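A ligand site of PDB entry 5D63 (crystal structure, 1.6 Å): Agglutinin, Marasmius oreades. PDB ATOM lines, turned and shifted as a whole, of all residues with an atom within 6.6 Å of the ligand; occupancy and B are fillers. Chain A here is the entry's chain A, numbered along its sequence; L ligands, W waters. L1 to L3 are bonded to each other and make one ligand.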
ATOM      1  N   HIS A   9       9.398 -24.256  -6.660  1.00  0.00           N
ATOM      2  CA  HIS A   9       8.511 -24.653  -7.764  1.00  0.00           C
ATOM      3  C   HIS A   9       7.613 -25.719  -7.168  1.00  0.00           C
ATOM      4  O   HIS A   9       8.124 -26.699  -6.599  1.00  0.00           O
ATOM      5  CB  HIS A   9       9.361 -25.213  -8.885  1.00  0.00           C
ATOM      6  CG  HIS A   9       8.581 -25.536 -10.121  1.00  0.00           C
ATOM      7  ND1 HIS A   9       8.272 -26.844 -10.516  1.00  0.00           N
ATOM      8  CD2 HIS A   9       7.959 -24.718 -11.010  1.00  0.00           C
ATOM      9  CE1 HIS A   9       7.506 -26.797 -11.570  1.00  0.00           C
ATOM     10  NE2 HIS A   9       7.326 -25.526 -11.916  1.00  0.00           N
ATOM     11  N   ASP A  20       0.666 -22.054 -10.735  1.00  0.00           N
ATOM     12  CA  ASP A  20       1.026 -21.064 -11.715  1.00  0.00           C
ATOM     13  C   ASP A  20       0.099 -19.823 -11.525  1.00  0.00           C
ATOM     14  O   ASP A  20      -1.111 -19.871 -11.438  1.00  0.00           O
ATOM     15  CB  ASP A  20       0.878 -21.765 -13.071  1.00  0.00           C
ATOM     16  CG  ASP A  20       1.189 -20.862 -14.303  1.00  0.00           C
ATOM     17  OD1 ASP A  20       0.565 -19.772 -14.496  1.00  0.00           O
ATOM     18  OD2 ASP A  20       2.066 -21.244 -15.128  1.00  0.00           O
ATOM     19  N   LEU A  21       0.709 -18.669 -11.449  1.00  0.00           N
ATOM     20  CA  LEU A  21      -0.034 -17.409 -11.417  1.00  0.00           C
ATOM     21  C   LEU A  21      -0.297 -17.008 -12.836  1.00  0.00           C
ATOM     22  O   LEU A  21       0.647 -16.736 -13.650  1.00  0.00           O
ATOM     23  CB  LEU A  21       0.797 -16.328 -10.736  1.00  0.00           C
ATOM     24  CG  LEU A  21       0.136 -14.973 -10.668  1.00  0.00           C
ATOM     25  CD1 LEU A  21      -1.184 -14.943  -9.857  1.00  0.00           C
ATOM     26  CD2 LEU A  21       1.071 -13.910 -10.055  1.00  0.00           C
ATOM     27  N   LYS A  22      -1.572 -17.017 -13.220  1.00  0.00           N
ATOM     28  CA  LYS A  22      -1.925 -17.030 -14.657  1.00  0.00           C
ATOM     29  C   LYS A  22      -1.387 -15.771 -15.369  1.00  0.00           C
ATOM     30  O   LYS A  22      -1.657 -14.619 -14.975  1.00  0.00           O
ATOM     31  CB  LYS A  22      -3.434 -17.178 -14.822  1.00  0.00           C
ATOM     32  CG  LYS A  22      -3.809 -17.767 -16.188  1.00  0.00           C
ATOM     33  CD  LYS A  22      -5.318 -17.923 -16.409  1.00  0.00           C
ATOM     34  CE  LYS A  22      -5.529 -18.490 -17.842  1.00  0.00           C
ATOM     35  NZ  LYS A  22      -7.015 -18.998 -17.911  1.00  0.00           N
ATOM     36  N   ASP A  23      -0.677 -15.974 -16.478  1.00  0.00           N
ATOM     37  CA  ASP A  23      -0.004 -14.927 -17.237  1.00  0.00           C
ATOM     38  C   ASP A  23       0.954 -14.056 -16.452  1.00  0.00           C
ATOM     39  O   ASP A  23       1.377 -13.032 -16.916  1.00  0.00           O
ATOM     40  CB  ASP A  23      -1.038 -14.080 -17.954  1.00  0.00           C
ATOM     41  CG  ASP A  23      -0.494 -13.476 -19.262  1.00  0.00           C
ATOM     42  OD1 ASP A  23       0.331 -14.112 -19.957  1.00  0.00           O
ATOM     43  OD2 ASP A  23      -0.820 -12.276 -19.498  1.00  0.00           O
ATOM     44  N   GLY A  24       1.391 -14.522 -15.302  1.00  0.00           N
ATOM     45  CA  GLY A  24       2.292 -13.761 -14.423  1.00  0.00           C
ATOM     46  C   GLY A  24       1.674 -12.447 -14.013  1.00  0.00           C
ATOM     47  O   GLY A  24       2.418 -11.574 -13.559  1.00  0.00           O
ATOM     48  N   VAL A  33      -3.506 -21.224 -10.909  1.00  0.00           N
ATOM     49  CA  VAL A  33      -4.036 -22.376 -11.599  1.00  0.00           C
ATOM     50  C   VAL A  33      -2.996 -23.477 -11.703  1.00  0.00           C
ATOM     51  O   VAL A  33      -1.780 -23.234 -11.589  1.00  0.00           O
ATOM     52  CB  VAL A  33      -4.461 -22.058 -13.071  1.00  0.00           C
ATOM     53  CG1 VAL A  33      -5.670 -21.121 -12.987  1.00  0.00           C
ATOM     54  CG2 VAL A  33      -3.332 -21.406 -13.819  1.00  0.00           C
ATOM     55  N   TRP A  35      -0.696 -25.861 -14.112  1.00  0.00           N
ATOM     56  CA  TRP A  35      -0.177 -25.665 -15.482  1.00  0.00           C
ATOM     57  C   TRP A  35       1.043 -26.622 -15.634  1.00  0.00           C
ATOM     58  O   TRP A  35       1.867 -26.712 -14.730  1.00  0.00           O
ATOM     59  CB  TRP A  35       0.257 -24.217 -15.671  1.00  0.00           C
ATOM     60  CG  TRP A  35       0.218 -23.774 -17.124  1.00  0.00           C
ATOM     61  CD1 TRP A  35       1.133 -24.068 -18.119  1.00  0.00           C
ATOM     62  CD2 TRP A  35      -0.818 -23.006 -17.757  1.00  0.00           C
ATOM     63  NE1 TRP A  35       0.736 -23.538 -19.321  1.00  0.00           N
ATOM     64  CE2 TRP A  35      -0.473 -22.890 -19.145  1.00  0.00           C
ATOM     65  CE3 TRP A  35      -2.017 -22.459 -17.309  1.00  0.00           C
ATOM     66  CZ2 TRP A  35      -1.262 -22.212 -20.057  1.00  0.00           C
ATOM     67  CZ3 TRP A  35      -2.819 -21.800 -18.246  1.00  0.00           C
ATOM     68  CH2 TRP A  35      -2.453 -21.711 -19.608  1.00  0.00           C
ATOM     69  N   GLN A  36       1.243 -27.142 -16.814  1.00  0.00           N
ATOM     70  CA  GLN A  36       2.408 -27.936 -17.077  1.00  0.00           C
ATOM     71  C   GLN A  36       3.680 -27.136 -17.052  1.00  0.00           C
ATOM     72  O   GLN A  36       3.664 -25.948 -17.199  1.00  0.00           O
ATOM     73  CB  GLN A  36       2.299 -28.668 -18.420  1.00  0.00           C
ATOM     74  CG  GLN A  36       2.335 -27.797 -19.656  1.00  0.00           C
ATOM     75  CD  GLN A  36       2.174 -28.655 -20.903  1.00  0.00           C
ATOM     76  OE1 GLN A  36       3.012 -29.483 -21.212  1.00  0.00           O
ATOM     77  NE2 GLN A  36       1.065 -28.522 -21.536  1.00  0.00           N
ATOM     78  N   PHE A  37       4.813 -27.817 -16.981  1.00  0.00           N
ATOM     79  CA  PHE A  37       6.090 -27.144 -16.809  1.00  0.00           C
ATOM     80  C   PHE A  37       7.208 -27.896 -17.514  1.00  0.00           C
ATOM     81  O   PHE A  37       6.996 -29.017 -17.957  1.00  0.00           O
ATOM     82  CB  PHE A  37       6.501 -27.048 -15.284  1.00  0.00           C
ATOM     83  CG  PHE A  37       6.722 -28.371 -14.587  1.00  0.00           C
ATOM     84  CD1 PHE A  37       5.676 -29.038 -14.009  1.00  0.00           C
ATOM     85  CD2 PHE A  37       7.983 -28.889 -14.468  1.00  0.00           C
ATOM     86  CE1 PHE A  37       5.860 -30.256 -13.356  1.00  0.00           C
ATOM     87  CE2 PHE A  37       8.212 -30.132 -13.819  1.00  0.00           C
ATOM     88  CZ  PHE A  37       7.123 -30.769 -13.288  1.00  0.00           C
ATOM     89  N   THR A  38       8.319 -27.192 -17.640  1.00  0.00           N
ATOM     90  CA  THR A  38       9.522 -27.804 -18.330  1.00  0.00           C
ATOM     91  C   THR A  38      10.643 -27.852 -17.316  1.00  0.00           C
ATOM     92  O   THR A  38      11.083 -26.833 -16.792  1.00  0.00           O
ATOM     93  CB  THR A  38       9.951 -26.950 -19.576  1.00  0.00           C
ATOM     94  OG1 THR A  38       8.793 -26.771 -20.452  1.00  0.00           O
ATOM     95  CG2 THR A  38      11.049 -27.662 -20.301  1.00  0.00           C
ATOM     96  N   PRO A  39      11.130 -29.044 -16.994  1.00  0.00           N
ATOM     97  CA  PRO A  39      12.241 -29.141 -16.009  1.00  0.00           C
ATOM     98  C   PRO A  39      13.499 -28.483 -16.507  1.00  0.00           C
ATOM     99  O   PRO A  39      13.714 -28.363 -17.710  1.00  0.00           O
ATOM    100  CB  PRO A  39      12.505 -30.630 -15.859  1.00  0.00           C
ATOM    101  CG  PRO A  39      11.578 -31.287 -16.804  1.00  0.00           C
ATOM    102  CD  PRO A  39      10.702 -30.337 -17.521  1.00  0.00           C
ATOM    103  N   THR A  41      14.428 -25.413 -16.604  1.00  0.00           N
ATOM    104  CA  THR A  41      14.180 -24.107 -17.199  1.00  0.00           C
ATOM    105  C   THR A  41      13.788 -23.171 -16.088  1.00  0.00           C
ATOM    106  O   THR A  41      13.438 -23.643 -15.013  1.00  0.00           O
ATOM    107  CB  THR A  41      13.050 -24.043 -18.251  1.00  0.00           C
ATOM    108  OG1 THR A  41      11.773 -24.238 -17.571  1.00  0.00           O
ATOM    109  CG2 THR A  41      13.248 -25.023 -19.349  1.00  0.00           C
ATOM    110  N   ILE A  42      13.846 -21.874 -16.329  1.00  0.00           N
ATOM    111  CA  ILE A  42      13.082 -20.945 -15.520  1.00  0.00           C
ATOM    112  C   ILE A  42      11.617 -21.038 -15.965  1.00  0.00           C
ATOM    113  O   ILE A  42      11.271 -20.673 -17.107  1.00  0.00           O
ATOM    114  CB  ILE A  42      13.585 -19.492 -15.639  1.00  0.00           C
ATOM    115  CG1 ILE A  42      15.064 -19.351 -15.144  1.00  0.00           C
ATOM    116  CG2 ILE A  42      12.578 -18.512 -14.988  1.00  0.00           C
ATOM    117  CD1 ILE A  42      15.323 -19.817 -13.752  1.00  0.00           C
ATOM    118  N   ASN A  43      10.745 -21.474 -15.040  1.00  0.00           N
ATOM    119  CA  ASN A  43       9.255 -21.471 -15.242  1.00  0.00           C
ATOM    120  C   ASN A  43       8.714 -20.177 -14.699  1.00  0.00           C
ATOM    121  O   ASN A  43       8.473 -20.033 -13.464  1.00  0.00           O
ATOM    122  CB  ASN A  43       8.631 -22.717 -14.568  1.00  0.00           C
ATOM    123  CG  ASN A  43       8.974 -23.993 -15.314  1.00  0.00           C
ATOM    124  OD1 ASN A  43       8.425 -24.276 -16.383  1.00  0.00           O
ATOM    125  ND2 ASN A  43       9.939 -24.735 -14.828  1.00  0.00           N
ATOM    126  N   TRP A  44       8.675 -19.165 -15.585  1.00  0.00           N
ATOM    127  CA  TRP A  44       8.516 -17.773 -15.241  1.00  0.00           C
ATOM    128  C   TRP A  44       7.334 -17.438 -14.339  1.00  0.00           C
ATOM    129  O   TRP A  44       7.443 -16.514 -13.481  1.00  0.00           O
ATOM    130  CB  TRP A  44       8.465 -16.915 -16.526  1.00  0.00           C
ATOM    131  CG  TRP A  44       9.792 -16.740 -17.145  1.00  0.00           C
ATOM    132  CD1 TRP A  44      10.367 -17.474 -18.163  1.00  0.00           C
ATOM    133  CD2 TRP A  44      10.791 -15.797 -16.721  1.00  0.00           C
ATOM    134  NE1 TRP A  44      11.614 -16.983 -18.428  1.00  0.00           N
ATOM    135  CE2 TRP A  44      11.919 -15.995 -17.536  1.00  0.00           C
ATOM    136  CE3 TRP A  44      10.799 -14.813 -15.765  1.00  0.00           C
ATOM    137  CZ2 TRP A  44      13.065 -15.219 -17.409  1.00  0.00           C
ATOM    138  CZ3 TRP A  44      11.933 -14.050 -15.622  1.00  0.00           C
ATOM    139  CH2 TRP A  44      13.074 -14.296 -16.416  1.00  0.00           C
ATOM    140  N   HIS A  45       6.199 -18.132 -14.464  1.00  0.00           N
ATOM    141  CA  HIS A  45       5.046 -17.807 -13.639  1.00  0.00           C
ATOM    142  C   HIS A  45       4.812 -18.705 -12.472  1.00  0.00           C
ATOM    143  O   HIS A  45       3.780 -18.643 -11.772  1.00  0.00           O
ATOM    144  CB  HIS A  45       3.775 -17.747 -14.542  1.00  0.00           C
ATOM    145  CG  HIS A  45       3.935 -16.829 -15.727  1.00  0.00           C
ATOM    146  ND1 HIS A  45       3.191 -16.974 -16.896  1.00  0.00           N
ATOM    147  CD2 HIS A  45       4.694 -15.742 -15.890  1.00  0.00           C
ATOM    148  CE1 HIS A  45       3.496 -15.982 -17.720  1.00  0.00           C
ATOM    149  NE2 HIS A  45       4.419 -15.232 -17.161  1.00  0.00           N
ATOM    150  N   GLN A  46       5.744 -19.618 -12.182  1.00  0.00           N
ATOM    151  CA  GLN A  46       5.572 -20.751 -11.279  1.00  0.00           C
ATOM    152  C   GLN A  46       6.608 -20.805 -10.158  1.00  0.00           C
ATOM    153  O   GLN A  46       6.847 -21.860  -9.601  1.00  0.00           O
ATOM    154  CB  GLN A  46       5.699 -22.050 -12.080  1.00  0.00           C
ATOM    155  CG  GLN A  46       4.700 -22.112 -13.242  1.00  0.00           C
ATOM    156  CD  GLN A  46       4.782 -23.402 -14.059  1.00  0.00           C
ATOM    157  OE1 GLN A  46       5.718 -24.221 -13.911  1.00  0.00           O
ATOM    158  NE2 GLN A  46       3.823 -23.571 -14.997  1.00  0.00           N
ATOM    159  N   PHE A  66       7.883 -13.529 -10.060  1.00  0.00           N
ATOM    160  CA  PHE A  66       7.669 -12.663 -11.239  1.00  0.00           C
ATOM    161  C   PHE A  66       6.747 -11.491 -10.953  1.00  0.00           C
ATOM    162  O   PHE A  66       7.119 -10.350 -11.262  1.00  0.00           O
ATOM    163  CB  PHE A  66       7.115 -13.479 -12.387  1.00  0.00           C
ATOM    164  CG  PHE A  66       6.960 -12.702 -13.661  1.00  0.00           C
ATOM    165  CD1 PHE A  66       8.090 -12.330 -14.431  1.00  0.00           C
ATOM    166  CD2 PHE A  66       5.711 -12.234 -14.058  1.00  0.00           C
ATOM    167  CE1 PHE A  66       7.949 -11.558 -15.561  1.00  0.00           C
ATOM    168  CE2 PHE A  66       5.553 -11.549 -15.254  1.00  0.00           C
ATOM    169  CZ  PHE A  66       6.666 -11.256 -16.034  1.00  0.00           C
ATOM    170  N   ASP A 131      -3.997 -27.499 -18.513  1.00  0.00           N
ATOM    171  CA  ASP A 131      -3.425 -26.187 -18.288  1.00  0.00           C
ATOM    172  C   ASP A 131      -4.552 -25.196 -17.991  1.00  0.00           C
ATOM    173  O   ASP A 131      -5.520 -25.011 -18.802  1.00  0.00           O
ATOM    174  CB  ASP A 131      -2.628 -25.739 -19.480  1.00  0.00           C
ATOM    175  CG  ASP A 131      -1.400 -26.611 -19.730  1.00  0.00           C
ATOM    176  OD1 ASP A 131      -0.905 -27.180 -18.772  1.00  0.00           O
ATOM    177  OD2 ASP A 131      -0.869 -26.596 -20.916  1.00  0.00           O
HETATM  178  C1  LIG L   1       5.968 -19.661 -21.181  1.00  0.00           C
HETATM  179  C2  LIG L   1       6.426 -19.754 -22.637  1.00  0.00           C
HETATM  180  C3  LIG L   1       6.255 -18.366 -23.314  1.00  0.00           C
HETATM  181  C4  LIG L   1       6.966 -17.307 -22.480  1.00  0.00           C
HETATM  182  C5  LIG L   1       6.346 -17.293 -21.063  1.00  0.00           C
HETATM  183  C6  LIG L   1       7.009 -16.251 -20.177  1.00  0.00           C
HETATM  184  O1  LIG L   1       5.613 -20.739 -23.275  1.00  0.00           O
HETATM  185  O2  LIG L   1       6.936 -18.529 -24.580  1.00  0.00           O
HETATM  186  O3  LIG L   1       8.414 -17.438 -22.410  1.00  0.00           O
HETATM  187  O4  LIG L   1       6.543 -18.577 -20.422  1.00  0.00           O
HETATM  188  C1  LG2 L   2       2.593 -18.499 -20.412  1.00  0.00           C
HETATM  189  C2  LG2 L   2       3.851 -19.284 -19.968  1.00  0.00           C
HETATM  190  C3  LG2 L   2       3.445 -20.669 -19.444  1.00  0.00           C
HETATM  191  C4  LG2 L   2       2.434 -20.619 -18.335  1.00  0.00           C
HETATM  192  C5  LG2 L   2       1.272 -19.647 -18.749  1.00  0.00           C
HETATM  193  C6  LG2 L   2       0.177 -19.417 -17.695  1.00  0.00           C
HETATM  194  O1  LG2 L   2       3.002 -17.146 -20.588  1.00  0.00           O
HETATM  195  O2  LG2 L   2       4.553 -19.477 -21.237  1.00  0.00           O
HETATM  196  O3  LG2 L   2       4.633 -21.400 -19.044  1.00  0.00           O
HETATM  197  O4  LG2 L   2       3.044 -20.045 -17.166  1.00  0.00           O
HETATM  198  O5  LG2 L   2       1.785 -18.359 -19.222  1.00  0.00           O
HETATM  199  O6  LG2 L   2       0.631 -18.497 -16.678  1.00  0.00           O
HETATM  200  C1  LG3 L   3       4.434 -22.751 -18.624  1.00  0.00           C
HETATM  201  C2  LG3 L   3       5.838 -23.338 -18.337  1.00  0.00           C
HETATM  202  C3  LG3 L   3       6.581 -23.738 -19.611  1.00  0.00           C
HETATM  203  C4  LG3 L   3       5.678 -24.537 -20.584  1.00  0.00           C
HETATM  204  C5  LG3 L   3       4.421 -23.704 -20.864  1.00  0.00           C
HETATM  205  C6  LG3 L   3       3.399 -24.309 -21.731  1.00  0.00           C
HETATM  206  O1  LG3 L   3       6.697 -22.540 -17.542  1.00  0.00           O
HETATM  207  O2  LG3 L   3       7.823 -24.466 -19.325  1.00  0.00           O
HETATM  208  O3  LG3 L   3       5.300 -25.771 -19.946  1.00  0.00           O
HETATM  209  O4  LG3 L   3       3.720 -23.507 -19.567  1.00  0.00           O
HETATM  210  O5  LG3 L   3       2.241 -23.439 -21.908  1.00  0.00           O
HETATM  211  O   HOH W   1       5.622 -20.275 -16.203  1.00  0.00           O
HETATM  212  O   HOH W   2       9.787 -22.797 -18.903  1.00  0.00           O
HETATM  213  O   HOH W   3      -0.406 -24.386 -22.776  1.00  0.00           O
HETATM  214  O   HOH W   4       8.398 -20.290 -18.458  1.00  0.00           O
HETATM  215  O   HOH W   5       2.799 -21.114 -23.328  1.00  0.00           O
HETATM  216  O   HOH W   6       6.773 -23.199 -23.356  1.00  0.00           O
HETATM  217  O   HOH W   7       9.609 -19.646 -20.984  1.00  0.00           O
HETATM  218  O   HOH W   8       7.638 -15.874 -25.511  1.00  0.00           O
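The side-chain carboxylate of Asp 20 lies within hydrogen-bond range of an oxygen (O6) of LG2 L2, 2.5 Å away. OD1 of Asn 43 is in hydrogen-bond range of O1 of LG3 L3, 2.7 Å away. An oxygen (O2) of LG3 L3 lies within hydrogen-bond range of the backbone NH (N) of Thr 38. O2 of LG3 L3 is in hydrogen-bond range of OG1 of Thr 38 (2.7 Å). An oxygen (O6) of LG2 L2 lies within hydrogen-bond range of the backbone NH of Asp 23, 2.8 Å away. ND1 of His 45 is in hydrogen-bond range of O6 of LG2 L2, 3.0 Å away. An oxygen (O4) of LG3 L3 lies within hydrogen-bond range of the indole nitrogen (NE1) of Trp 35 (3.0 Å). An oxygen (O3) of LG3 L3 is in hydrogen-bond range of the backbone carbonyl oxygen (O) of Gln 36 (3.2 Å).
The side-chain amide nitrogen (NE2) of Gln 46 is in hydrogen-bond range of the side-chain carboxylate (OD2) of Asp 20, 2.9 Å away. O of Thr 38 lies within hydrogen-bond range of ND2 of Asn 43 (3.1 Å). The side-chain hydroxyl of Thr 41 lies within hydrogen-bond range of the side-chain amide nitrogen of Asn 43, at 3.3 Å. The side-chain hydroxyl of Thr 41 sits at hydrogen-bond distance from the backbone carbonyl oxygen of Thr 38 (2.8 Å). O of His 45 is in hydrogen-bond range of N of Leu 21, at 3.1 Å. The backbone NH (N) of Gly 24 lies within hydrogen-bond range of a ring nitrogen (ND1) of His 45 (3.4 Å). O of Gln 36 sits at hydrogen-bond distance from NE2 of Gln 46 (3.2 Å). The side-chain amide nitrogen of Gln 36 lies within hydrogen-bond range of the side-chain carboxylate of Asp 131 (2.8 Å).
Merely in contact with the ligand: Leu 21 (3.5 Å), Phe 37 (3.5 Å), Lys 22 (3.6 Å), Gln 46 (3.8 Å) and Trp 44 (3.99 Å). Of the 20 residues printed, 12 come within 4 Å of the ligand. The nearest printed residue that does not touch the ligand is Gly 24 (4.3 Å).
Water W2 lies within hydrogen-bond range of O2 of LG3 L3 (2.6 Å), OG1 of Thr 41 (2.8 Å), O of Ile 42 (3.2 Å) and OD1 of Asn 43 (3.2 Å). Water W1 lies within hydrogen-bond range of O4 of LG2 L2 (2.8 Å), N of His 45 (2.8 Å) and N of Trp 44 (3.3 Å). Water W3 bridges OD2 of Asp 131 (2.9 Å) and O5 of LG3 L3 (2.9 Å). Water W4 lies within hydrogen-bond range of O1 of LG3 L3 (3.0 Å), N of Trp 44 (3.1 Å) and O of Ile 42 (3.2 Å).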
